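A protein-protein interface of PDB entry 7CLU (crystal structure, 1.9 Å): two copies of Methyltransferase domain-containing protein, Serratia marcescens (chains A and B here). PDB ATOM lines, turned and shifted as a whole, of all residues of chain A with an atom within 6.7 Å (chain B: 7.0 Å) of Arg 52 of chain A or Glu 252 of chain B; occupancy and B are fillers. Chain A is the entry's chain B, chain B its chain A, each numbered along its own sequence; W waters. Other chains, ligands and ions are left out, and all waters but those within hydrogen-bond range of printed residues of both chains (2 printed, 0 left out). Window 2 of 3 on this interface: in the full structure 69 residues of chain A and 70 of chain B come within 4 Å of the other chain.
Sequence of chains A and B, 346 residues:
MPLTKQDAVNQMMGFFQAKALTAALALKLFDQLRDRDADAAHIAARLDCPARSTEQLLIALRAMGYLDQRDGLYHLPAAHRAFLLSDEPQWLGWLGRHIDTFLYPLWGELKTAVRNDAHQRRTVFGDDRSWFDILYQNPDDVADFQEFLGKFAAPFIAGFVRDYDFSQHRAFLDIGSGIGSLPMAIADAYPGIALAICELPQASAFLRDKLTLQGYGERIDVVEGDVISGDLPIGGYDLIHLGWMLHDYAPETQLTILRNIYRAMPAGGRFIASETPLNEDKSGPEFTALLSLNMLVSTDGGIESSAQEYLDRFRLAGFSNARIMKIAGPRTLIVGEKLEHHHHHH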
ATOM      1  N   ALA A  44      -2.064 -34.688  19.305  1.00  0.00           N
ATOM      2  CA  ALA A  44      -3.482 -34.401  19.508  1.00  0.00           C
ATOM      3  C   ALA A  44      -4.139 -35.424  20.431  1.00  0.00           C
ATOM      4  O   ALA A  44      -4.889 -35.060  21.345  1.00  0.00           O
ATOM      5  CB  ALA A  44      -4.207 -34.360  18.163  1.00  0.00           C
ATOM      6  N   CYS A  49      -7.429 -33.466  22.152  1.00  0.00           N
ATOM      7  CA  CYS A  49      -7.793 -32.475  21.156  1.00  0.00           C
ATOM      8  C   CYS A  49      -7.897 -33.126  19.783  1.00  0.00           C
ATOM      9  O   CYS A  49      -7.195 -34.095  19.503  1.00  0.00           O
ATOM     10  CB  CYS A  49      -6.746 -31.351  21.085  1.00  0.00           C
ATOM     11  SG  CYS A  49      -6.668 -30.261  22.478  1.00  0.00           S
ATOM     12  N   PRO A  50      -8.723 -32.585  18.891  1.00  0.00           N
ATOM     13  CA  PRO A  50      -8.784 -33.124  17.526  1.00  0.00           C
ATOM     14  C   PRO A  50      -7.493 -32.870  16.758  1.00  0.00           C
ATOM     15  O   PRO A  50      -6.766 -31.897  17.006  1.00  0.00           O
ATOM     16  CB  PRO A  50      -9.969 -32.375  16.894  1.00  0.00           C
ATOM     17  CG  PRO A  50     -10.753 -31.831  18.041  1.00  0.00           C
ATOM     18  CD  PRO A  50      -9.743 -31.553  19.125  1.00  0.00           C
ATOM     19  N   ALA A  51      -7.209 -33.779  15.815  1.00  0.00           N
ATOM     20  CA  ALA A  51      -5.936 -33.735  15.096  1.00  0.00           C
ATOM     21  C   ALA A  51      -5.843 -32.525  14.179  1.00  0.00           C
ATOM     22  O   ALA A  51      -4.776 -31.908  14.065  1.00  0.00           O
ATOM     23  CB  ALA A  51      -5.732 -35.010  14.282  1.00  0.00           C
ATOM     24  N   ARG A  52      -6.937 -32.185  13.492  1.00  0.00           N
ATOM     25  CA  ARG A  52      -6.899 -31.055  12.566  1.00  0.00           C
ATOM     26  C   ARG A  52      -6.531 -29.756  13.284  1.00  0.00           C
ATOM     27  O   ARG A  52      -5.634 -29.033  12.849  1.00  0.00           O
ATOM     28  CB  ARG A  52      -8.242 -30.920  11.850  1.00  0.00           C
ATOM     29  CG  ARG A  52      -8.296 -29.778  10.855  1.00  0.00           C
ATOM     30  CD  ARG A  52      -9.643 -29.755  10.118  1.00  0.00           C
ATOM     31  NE  ARG A  52      -9.783 -30.844   9.155  1.00  0.00           N
ATOM     32  CZ  ARG A  52     -10.533 -30.777   8.059  1.00  0.00           C
ATOM     33  NH1 ARG A  52     -11.210 -29.669   7.785  1.00  0.00           N
ATOM     34  NH2 ARG A  52     -10.614 -31.817   7.237  1.00  0.00           N
ATOM     35  N   SER A  53      -7.204 -29.448  14.399  1.00  0.00           N
ATOM     36  CA  SER A  53      -6.941 -28.173  15.067  1.00  0.00           C
ATOM     37  C   SER A  53      -5.582 -28.173  15.757  1.00  0.00           C
ATOM     38  O   SER A  53      -4.877 -27.155  15.749  1.00  0.00           O
ATOM     39  CB  SER A  53      -8.056 -27.859  16.063  1.00  0.00           C
ATOM     40  OG  SER A  53      -8.315 -28.969  16.906  1.00  0.00           O
ATOM     41  N   THR A  54      -5.188 -29.298  16.357  1.00  0.00           N
ATOM     42  CA  THR A  54      -3.857 -29.369  16.957  1.00  0.00           C
ATOM     43  C   THR A  54      -2.774 -29.193  15.896  1.00  0.00           C
ATOM     44  O   THR A  54      -1.771 -28.506  16.126  1.00  0.00           O
ATOM     45  CB  THR A  54      -3.674 -30.700  17.692  1.00  0.00           C
ATOM     46  OG1 THR A  54      -4.801 -30.945  18.539  1.00  0.00           O
ATOM     47  CG2 THR A  54      -2.413 -30.671  18.536  1.00  0.00           C
ATOM     48  N   GLU A  55      -2.965 -29.803  14.724  1.00  0.00           N
ATOM     49  CA  GLU A  55      -1.987 -29.659  13.649  1.00  0.00           C
ATOM     50  C   GLU A  55      -1.838 -28.204  13.217  1.00  0.00           C
ATOM     51  O   GLU A  55      -0.719 -27.737  12.967  1.00  0.00           O
ATOM     52  CB  GLU A  55      -2.379 -30.518  12.450  1.00  0.00           C
ATOM     53  CG  GLU A  55      -1.467 -30.238  11.250  1.00  0.00           C
ATOM     54  CD  GLU A  55      -1.506 -31.320  10.193  1.00  0.00           C
ATOM     55  OE1 GLU A  55      -2.618 -31.632   9.710  1.00  0.00           O
ATOM     56  OE2 GLU A  55      -0.420 -31.837   9.830  1.00  0.00           O
ATOM     57  N   GLN A  56      -2.954 -27.469  13.130  1.00  0.00           N
ATOM     58  CA  GLN A  56      -2.861 -26.040  12.844  1.00  0.00           C
ATOM     59  C   GLN A  56      -2.008 -25.314  13.878  1.00  0.00           C
ATOM     60  O   GLN A  56      -1.178 -24.471  13.523  1.00  0.00           O
ATOM     61  CB  GLN A  56      -4.248 -25.417  12.778  1.00  0.00           C
ATOM     62  CG  GLN A  56      -5.056 -25.919  11.610  1.00  0.00           C
ATOM     63  CD  GLN A  56      -6.463 -25.388  11.613  1.00  0.00           C
ATOM     64  OE1 GLN A  56      -7.368 -25.989  12.207  1.00  0.00           O
ATOM     65  NE2 GLN A  56      -6.666 -24.256  10.943  1.00  0.00           N
ATOM     66  N   LEU A  57      -2.223 -25.592  15.165  1.00  0.00           N
ATOM     67  CA  LEU A  57      -1.403 -24.940  16.187  1.00  0.00           C
ATOM     68  C   LEU A  57       0.049 -25.411  16.114  1.00  0.00           C
ATOM     69  O   LEU A  57       0.973 -24.617  16.321  1.00  0.00           O
ATOM     70  CB  LEU A  57      -1.987 -25.183  17.578  1.00  0.00           C
ATOM     71  CG  LEU A  57      -1.223 -24.587  18.759  1.00  0.00           C
ATOM     72  CD1 LEU A  57      -0.973 -23.068  18.566  1.00  0.00           C
ATOM     73  CD2 LEU A  57      -1.952 -24.876  20.065  1.00  0.00           C
ATOM     74  N   VAL B 114      -8.873 -24.766  19.617  1.00  0.00           N
ATOM     75  CA  VAL B 114      -8.049 -25.924  19.305  1.00  0.00           C
ATOM     76  C   VAL B 114      -8.594 -27.156  20.011  1.00  0.00           C
ATOM     77  O   VAL B 114      -8.566 -28.266  19.467  1.00  0.00           O
ATOM     78  CB  VAL B 114      -6.576 -25.663  19.677  1.00  0.00           C
ATOM     79  CG1 VAL B 114      -5.737 -26.909  19.406  1.00  0.00           C
ATOM     80  CG2 VAL B 114      -6.017 -24.492  18.875  1.00  0.00           C
ATOM     81  N   ASP B 117     -11.814 -27.816  17.838  1.00  0.00           N
ATOM     82  CA  ASP B 117     -11.747 -27.576  16.397  1.00  0.00           C
ATOM     83  C   ASP B 117     -13.019 -26.902  15.889  1.00  0.00           C
ATOM     84  O   ASP B 117     -13.694 -27.383  14.980  1.00  0.00           O
ATOM     85  CB  ASP B 117     -11.465 -28.857  15.624  1.00  0.00           C
ATOM     86  CG  ASP B 117     -11.278 -28.602  14.143  1.00  0.00           C
ATOM     87  OD1 ASP B 117     -10.714 -27.541  13.783  1.00  0.00           O
ATOM     88  OD2 ASP B 117     -11.714 -29.445  13.337  1.00  0.00           O
ATOM     89  N   TYR B 249     -13.217 -21.999   3.628  1.00  0.00           N
ATOM     90  CA  TYR B 249     -14.147 -23.106   3.795  1.00  0.00           C
ATOM     91  C   TYR B 249     -13.412 -24.400   4.115  1.00  0.00           C
ATOM     92  O   TYR B 249     -12.233 -24.578   3.798  1.00  0.00           O
ATOM     93  CB  TYR B 249     -15.000 -23.298   2.533  1.00  0.00           C
ATOM     94  CG  TYR B 249     -15.783 -22.056   2.203  1.00  0.00           C
ATOM     95  CD1 TYR B 249     -16.943 -21.735   2.907  1.00  0.00           C
ATOM     96  CD2 TYR B 249     -15.336 -21.169   1.232  1.00  0.00           C
ATOM     97  CE1 TYR B 249     -17.648 -20.580   2.627  1.00  0.00           C
ATOM     98  CE2 TYR B 249     -16.031 -20.014   0.949  1.00  0.00           C
ATOM     99  CZ  TYR B 249     -17.183 -19.722   1.652  1.00  0.00           C
ATOM    100  OH  TYR B 249     -17.875 -18.569   1.371  1.00  0.00           O
ATOM    101  N   ALA B 250     -14.137 -25.314   4.753  1.00  0.00           N
ATOM    102  CA  ALA B 250     -13.609 -26.646   4.970  1.00  0.00           C
ATOM    103  C   ALA B 250     -13.314 -27.310   3.625  1.00  0.00           C
ATOM    104  O   ALA B 250     -13.951 -26.997   2.611  1.00  0.00           O
ATOM    105  CB  ALA B 250     -14.598 -27.500   5.768  1.00  0.00           C
ATOM    106  N   PRO B 251     -12.346 -28.224   3.594  1.00  0.00           N
ATOM    107  CA  PRO B 251     -12.034 -28.943   2.343  1.00  0.00           C
ATOM    108  C   PRO B 251     -13.237 -29.557   1.647  1.00  0.00           C
ATOM    109  O   PRO B 251     -13.325 -29.492   0.410  1.00  0.00           O
ATOM    110  CB  PRO B 251     -11.048 -30.018   2.820  1.00  0.00           C
ATOM    111  CG  PRO B 251     -10.344 -29.363   3.970  1.00  0.00           C
ATOM    112  CD  PRO B 251     -11.393 -28.540   4.671  1.00  0.00           C
ATOM    113  N   GLU B 252     -14.162 -30.160   2.407  1.00  0.00           N
ATOM    114  CA  GLU B 252     -15.348 -30.755   1.799  1.00  0.00           C
ATOM    115  C   GLU B 252     -16.191 -29.699   1.094  1.00  0.00           C
ATOM    116  O   GLU B 252     -16.724 -29.944   0.007  1.00  0.00           O
ATOM    117  CB  GLU B 252     -16.172 -31.494   2.866  1.00  0.00           C
ATOM    118  CG  GLU B 252     -15.337 -32.278   3.891  1.00  0.00           C
ATOM    119  CD  GLU B 252     -14.666 -31.384   4.951  1.00  0.00           C
ATOM    120  OE1 GLU B 252     -15.381 -30.626   5.631  1.00  0.00           O
ATOM    121  OE2 GLU B 252     -13.425 -31.439   5.103  1.00  0.00           O
ATOM    122  N   THR B 253     -16.309 -28.510   1.688  1.00  0.00           N
ATOM    123  CA  THR B 253     -16.988 -27.412   1.006  1.00  0.00           C
ATOM    124  C   THR B 253     -16.166 -26.908  -0.173  1.00  0.00           C
ATOM    125  O   THR B 253     -16.719 -26.528  -1.217  1.00  0.00           O
ATOM    126  CB  THR B 253     -17.253 -26.283   1.999  1.00  0.00           C
ATOM    127  OG1 THR B 253     -18.046 -26.795   3.081  1.00  0.00           O
ATOM    128  CG2 THR B 253     -17.967 -25.099   1.323  1.00  0.00           C
ATOM    129  N   GLN B 254     -14.842 -26.878  -0.023  1.00  0.00           N
ATOM    130  CA  GLN B 254     -14.002 -26.510  -1.157  1.00  0.00           C
ATOM    131  C   GLN B 254     -14.281 -27.423  -2.343  1.00  0.00           C
ATOM    132  O   GLN B 254     -14.386 -26.963  -3.488  1.00  0.00           O
ATOM    133  CB  GLN B 254     -12.528 -26.575  -0.769  1.00  0.00           C
ATOM    134  CG  GLN B 254     -12.118 -25.624   0.341  1.00  0.00           C
ATOM    135  CD  GLN B 254     -10.623 -25.633   0.546  1.00  0.00           C
ATOM    136  OE1 GLN B 254      -9.861 -25.965  -0.373  1.00  0.00           O
ATOM    137  NE2 GLN B 254     -10.179 -25.263   1.755  1.00  0.00           N
ATOM    138  N   LEU B 255     -14.435 -28.718  -2.074  1.00  0.00           N
ATOM    139  CA  LEU B 255     -14.747 -29.673  -3.132  1.00  0.00           C
ATOM    140  C   LEU B 255     -16.072 -29.332  -3.806  1.00  0.00           C
ATOM    141  O   LEU B 255     -16.191 -29.413  -5.035  1.00  0.00           O
ATOM    142  CB  LEU B 255     -14.783 -31.081  -2.543  1.00  0.00           C
ATOM    143  CG  LEU B 255     -14.103 -32.236  -3.256  1.00  0.00           C
ATOM    144  CD1 LEU B 255     -12.613 -31.937  -3.433  1.00  0.00           C
ATOM    145  CD2 LEU B 255     -14.313 -33.515  -2.460  1.00  0.00           C
ATOM    146  N   THR B 256     -17.076 -28.941  -3.015  1.00  0.00           N
ATOM    147  CA  THR B 256     -18.378 -28.598  -3.581  1.00  0.00           C
ATOM    148  C   THR B 256     -18.274 -27.380  -4.493  1.00  0.00           C
ATOM    149  O   THR B 256     -18.795 -27.379  -5.617  1.00  0.00           O
ATOM    150  CB  THR B 256     -19.387 -28.340  -2.461  1.00  0.00           C
ATOM    151  OG1 THR B 256     -19.625 -29.554  -1.737  1.00  0.00           O
ATOM    152  CG2 THR B 256     -20.678 -27.816  -3.036  1.00  0.00           C
ATOM    153  N   ILE B 257     -17.603 -26.327  -4.013  1.00  0.00           N
ATOM    154  CA  ILE B 257     -17.373 -25.132  -4.825  1.00  0.00           C
ATOM    155  C   ILE B 257     -16.674 -25.499  -6.130  1.00  0.00           C
ATOM    156  O   ILE B 257     -17.069 -25.053  -7.215  1.00  0.00           O
ATOM    157  CB  ILE B 257     -16.545 -24.108  -4.027  1.00  0.00           C
ATOM    158  CG1 ILE B 257     -17.380 -23.484  -2.904  1.00  0.00           C
ATOM    159  CG2 ILE B 257     -15.998 -23.065  -4.951  1.00  0.00           C
ATOM    160  CD1 ILE B 257     -16.553 -22.981  -1.737  1.00  0.00           C
ATOM    161  N   ARG B 259     -16.342 -28.456  -7.668  1.00  0.00           N
ATOM    162  CA  ARG B 259     -17.215 -29.251  -8.522  1.00  0.00           C
ATOM    163  C   ARG B 259     -18.300 -28.380  -9.141  1.00  0.00           C
ATOM    164  O   ARG B 259     -18.662 -28.559 -10.308  1.00  0.00           O
ATOM    165  CB  ARG B 259     -17.823 -30.403  -7.714  1.00  0.00           C
ATOM    166  CG  ARG B 259     -16.847 -31.540  -7.420  1.00  0.00           C
ATOM    167  CD  ARG B 259     -17.576 -32.852  -7.101  1.00  0.00           C
ATOM    168  NE  ARG B 259     -18.223 -32.801  -5.797  1.00  0.00           N
ATOM    169  CZ  ARG B 259     -17.755 -33.409  -4.710  1.00  0.00           C
ATOM    170  NH1 ARG B 259     -16.639 -34.124  -4.790  1.00  0.00           N
ATOM    171  NH2 ARG B 259     -18.406 -33.311  -3.549  1.00  0.00           N
ATOM    172  N   LEU B 296      -9.554 -20.896  11.926  1.00  0.00           N
ATOM    173  CA  LEU B 296     -10.090 -21.811  12.922  1.00  0.00           C
ATOM    174  C   LEU B 296     -11.003 -21.086  13.903  1.00  0.00           C
ATOM    175  O   LEU B 296     -12.117 -21.548  14.186  1.00  0.00           O
ATOM    176  CB  LEU B 296      -8.938 -22.496  13.664  1.00  0.00           C
ATOM    177  CG  LEU B 296      -9.276 -23.238  14.951  1.00  0.00           C
ATOM    178  CD1 LEU B 296     -10.170 -24.440  14.620  1.00  0.00           C
ATOM    179  CD2 LEU B 296      -7.995 -23.695  15.655  1.00  0.00           C
ATOM    180  N   GLY B 301     -15.052 -23.688   9.144  1.00  0.00           N
ATOM    181  CA  GLY B 301     -14.092 -24.749   8.898  1.00  0.00           C
ATOM    182  C   GLY B 301     -12.936 -24.350   8.003  1.00  0.00           C
ATOM    183  O   GLY B 301     -12.217 -25.212   7.478  1.00  0.00           O
ATOM    184  N   GLY B 302     -12.739 -23.045   7.834  1.00  0.00           N
ATOM    185  CA  GLY B 302     -11.622 -22.572   7.037  1.00  0.00           C
ATOM    186  C   GLY B 302     -10.288 -23.053   7.575  1.00  0.00           C
ATOM    187  O   GLY B 302     -10.116 -23.295   8.779  1.00  0.00           O
ATOM    188  N   ILE B 303      -9.322 -23.157   6.658  1.00  0.00           N
ATOM    189  CA  ILE B 303      -8.010 -23.740   6.903  1.00  0.00           C
ATOM    190  C   ILE B 303      -7.111 -23.395   5.714  1.00  0.00           C
ATOM    191  O   ILE B 303      -7.601 -23.163   4.607  1.00  0.00           O
ATOM    192  CB  ILE B 303      -8.120 -25.261   7.102  1.00  0.00           C
ATOM    193  CG1 ILE B 303      -6.821 -25.852   7.656  1.00  0.00           C
ATOM    194  CG2 ILE B 303      -8.496 -25.964   5.786  1.00  0.00           C
ATOM    195  CD1 ILE B 303      -7.025 -27.122   8.519  1.00  0.00           C
ATOM    196  N   ARG B 313      -7.500 -31.571  -4.541  1.00  0.00           N
ATOM    197  CA  ARG B 313      -8.901 -31.166  -4.580  1.00  0.00           C
ATOM    198  C   ARG B 313      -9.332 -30.786  -5.989  1.00  0.00           C
ATOM    199  O   ARG B 313     -10.470 -31.066  -6.385  1.00  0.00           O
ATOM    200  CB  ARG B 313      -9.150 -30.014  -3.599  1.00  0.00           C
ATOM    201  CG  ARG B 313      -9.137 -30.479  -2.170  1.00  0.00           C
ATOM    202  CD  ARG B 313      -9.329 -29.377  -1.125  1.00  0.00           C
ATOM    203  NE  ARG B 313      -8.727 -29.841   0.123  1.00  0.00           N
ATOM    204  CZ  ARG B 313      -8.034 -29.071   0.943  1.00  0.00           C
ATOM    205  NH1 ARG B 313      -7.874 -27.782   0.659  1.00  0.00           N
ATOM    206  NH2 ARG B 313      -7.506 -29.589   2.042  1.00  0.00           N
HETATM  207  O   HOH W   1      -9.874 -26.772  11.527  1.00  0.00           O
HETATM  208  O   HOH W   2     -11.383 -27.519   8.882  1.00  0.00           O
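Cys 49 of chain A touches Val 114 of chain B.
Pro 50 of chain A touches Val 114 of chain B (CD to O, 3.5 Å).
Pro 50 of chain A touches Asp 117 of chain B.
CD of Arg 52 of chain A touches OD2 of Asp 117 of chain B (3.8 Å).
Arg 52 of chain A touches Pro 251 of chain B.
Ile 303 of chain B touches Arg 52 of chain A.
Ser 53 of chain A touches Asp 117 of chain B (OG to CB, 3.4 Å).
Val 114 of chain B touches Thr 54 of chain A.
Leu 296 of chain B touches Gln 56 of chain A.
Gln 56 of chain A touches Ile 303 of chain B (CD to CD1, 3.6 Å).
Of the 17 printed residues of chain B, 6 touch a printed residue of chain A.
Among the printed residues, 12 pairs touch across the chains.
O of Pro 50 of chain A is in hydrogen-bond range of OG1 of Thr 54 of chain A, at 2.7 Å.
The backbone carbonyl oxygen (O) of Ala 44 of chain A lies within hydrogen-bond range of the backbone NH (N) of Cys 49 of chain A (3.1 Å).
OG of Ser 53 of chain A sits at hydrogen-bond distance from O of Pro 50 of chain A (3.3 Å).
The backbone carbonyl oxygen (O) of Glu 252 of chain B is in hydrogen-bond range of the side-chain hydroxyl (OG1) of Thr 256 of chain B, 3.4 Å away.
The side-chain carboxylate of Glu 252 of chain B is in salt-bridge range of the guanidinium group of Arg 52 of chain A, 3.5 Å away.
The backbone carbonyl oxygen of Val 114 of chain B lies within hydrogen-bond range of the side-chain hydroxyl of Ser 53 of chain A (2.7 Å).
Of the printed residues of chain B, Cys 49 of chain A touches Val 114.
Printed residues of chain B within 4 Å of Arg 52 of chain A: Asp 117, Pro 251, Glu 252 and Ile 303.
Printed residues of chain B within 4 Å of Thr 54 of chain A: Val 114.
Printed residues of chain A within 4 Å of Asp 117 of chain B: Pro 50, Arg 52 and Ser 53.
Of the printed residues of chain A, Leu 296 of chain B touches Gln 56 (3.96 Å).
Of the printed residues of chain A, Ile 303 of chain B touches Arg 52 and Gln 56.
No position is printed for both chains.
Of the 12 pairs that touch across the chains among the printed residues, none has its exchanged pair printed and touching as well.
Water W2 lies within hydrogen-bond range of the guanidinium group of Arg 52 of chain A and the backbone carbonyl oxygen of Gly 301 of chain B.
Water W1 lies within hydrogen-bond range of OD1 of Asp 117 of chain B (2.5 Å) and OE1 of Gln 56 of chain A (2.7 Å).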
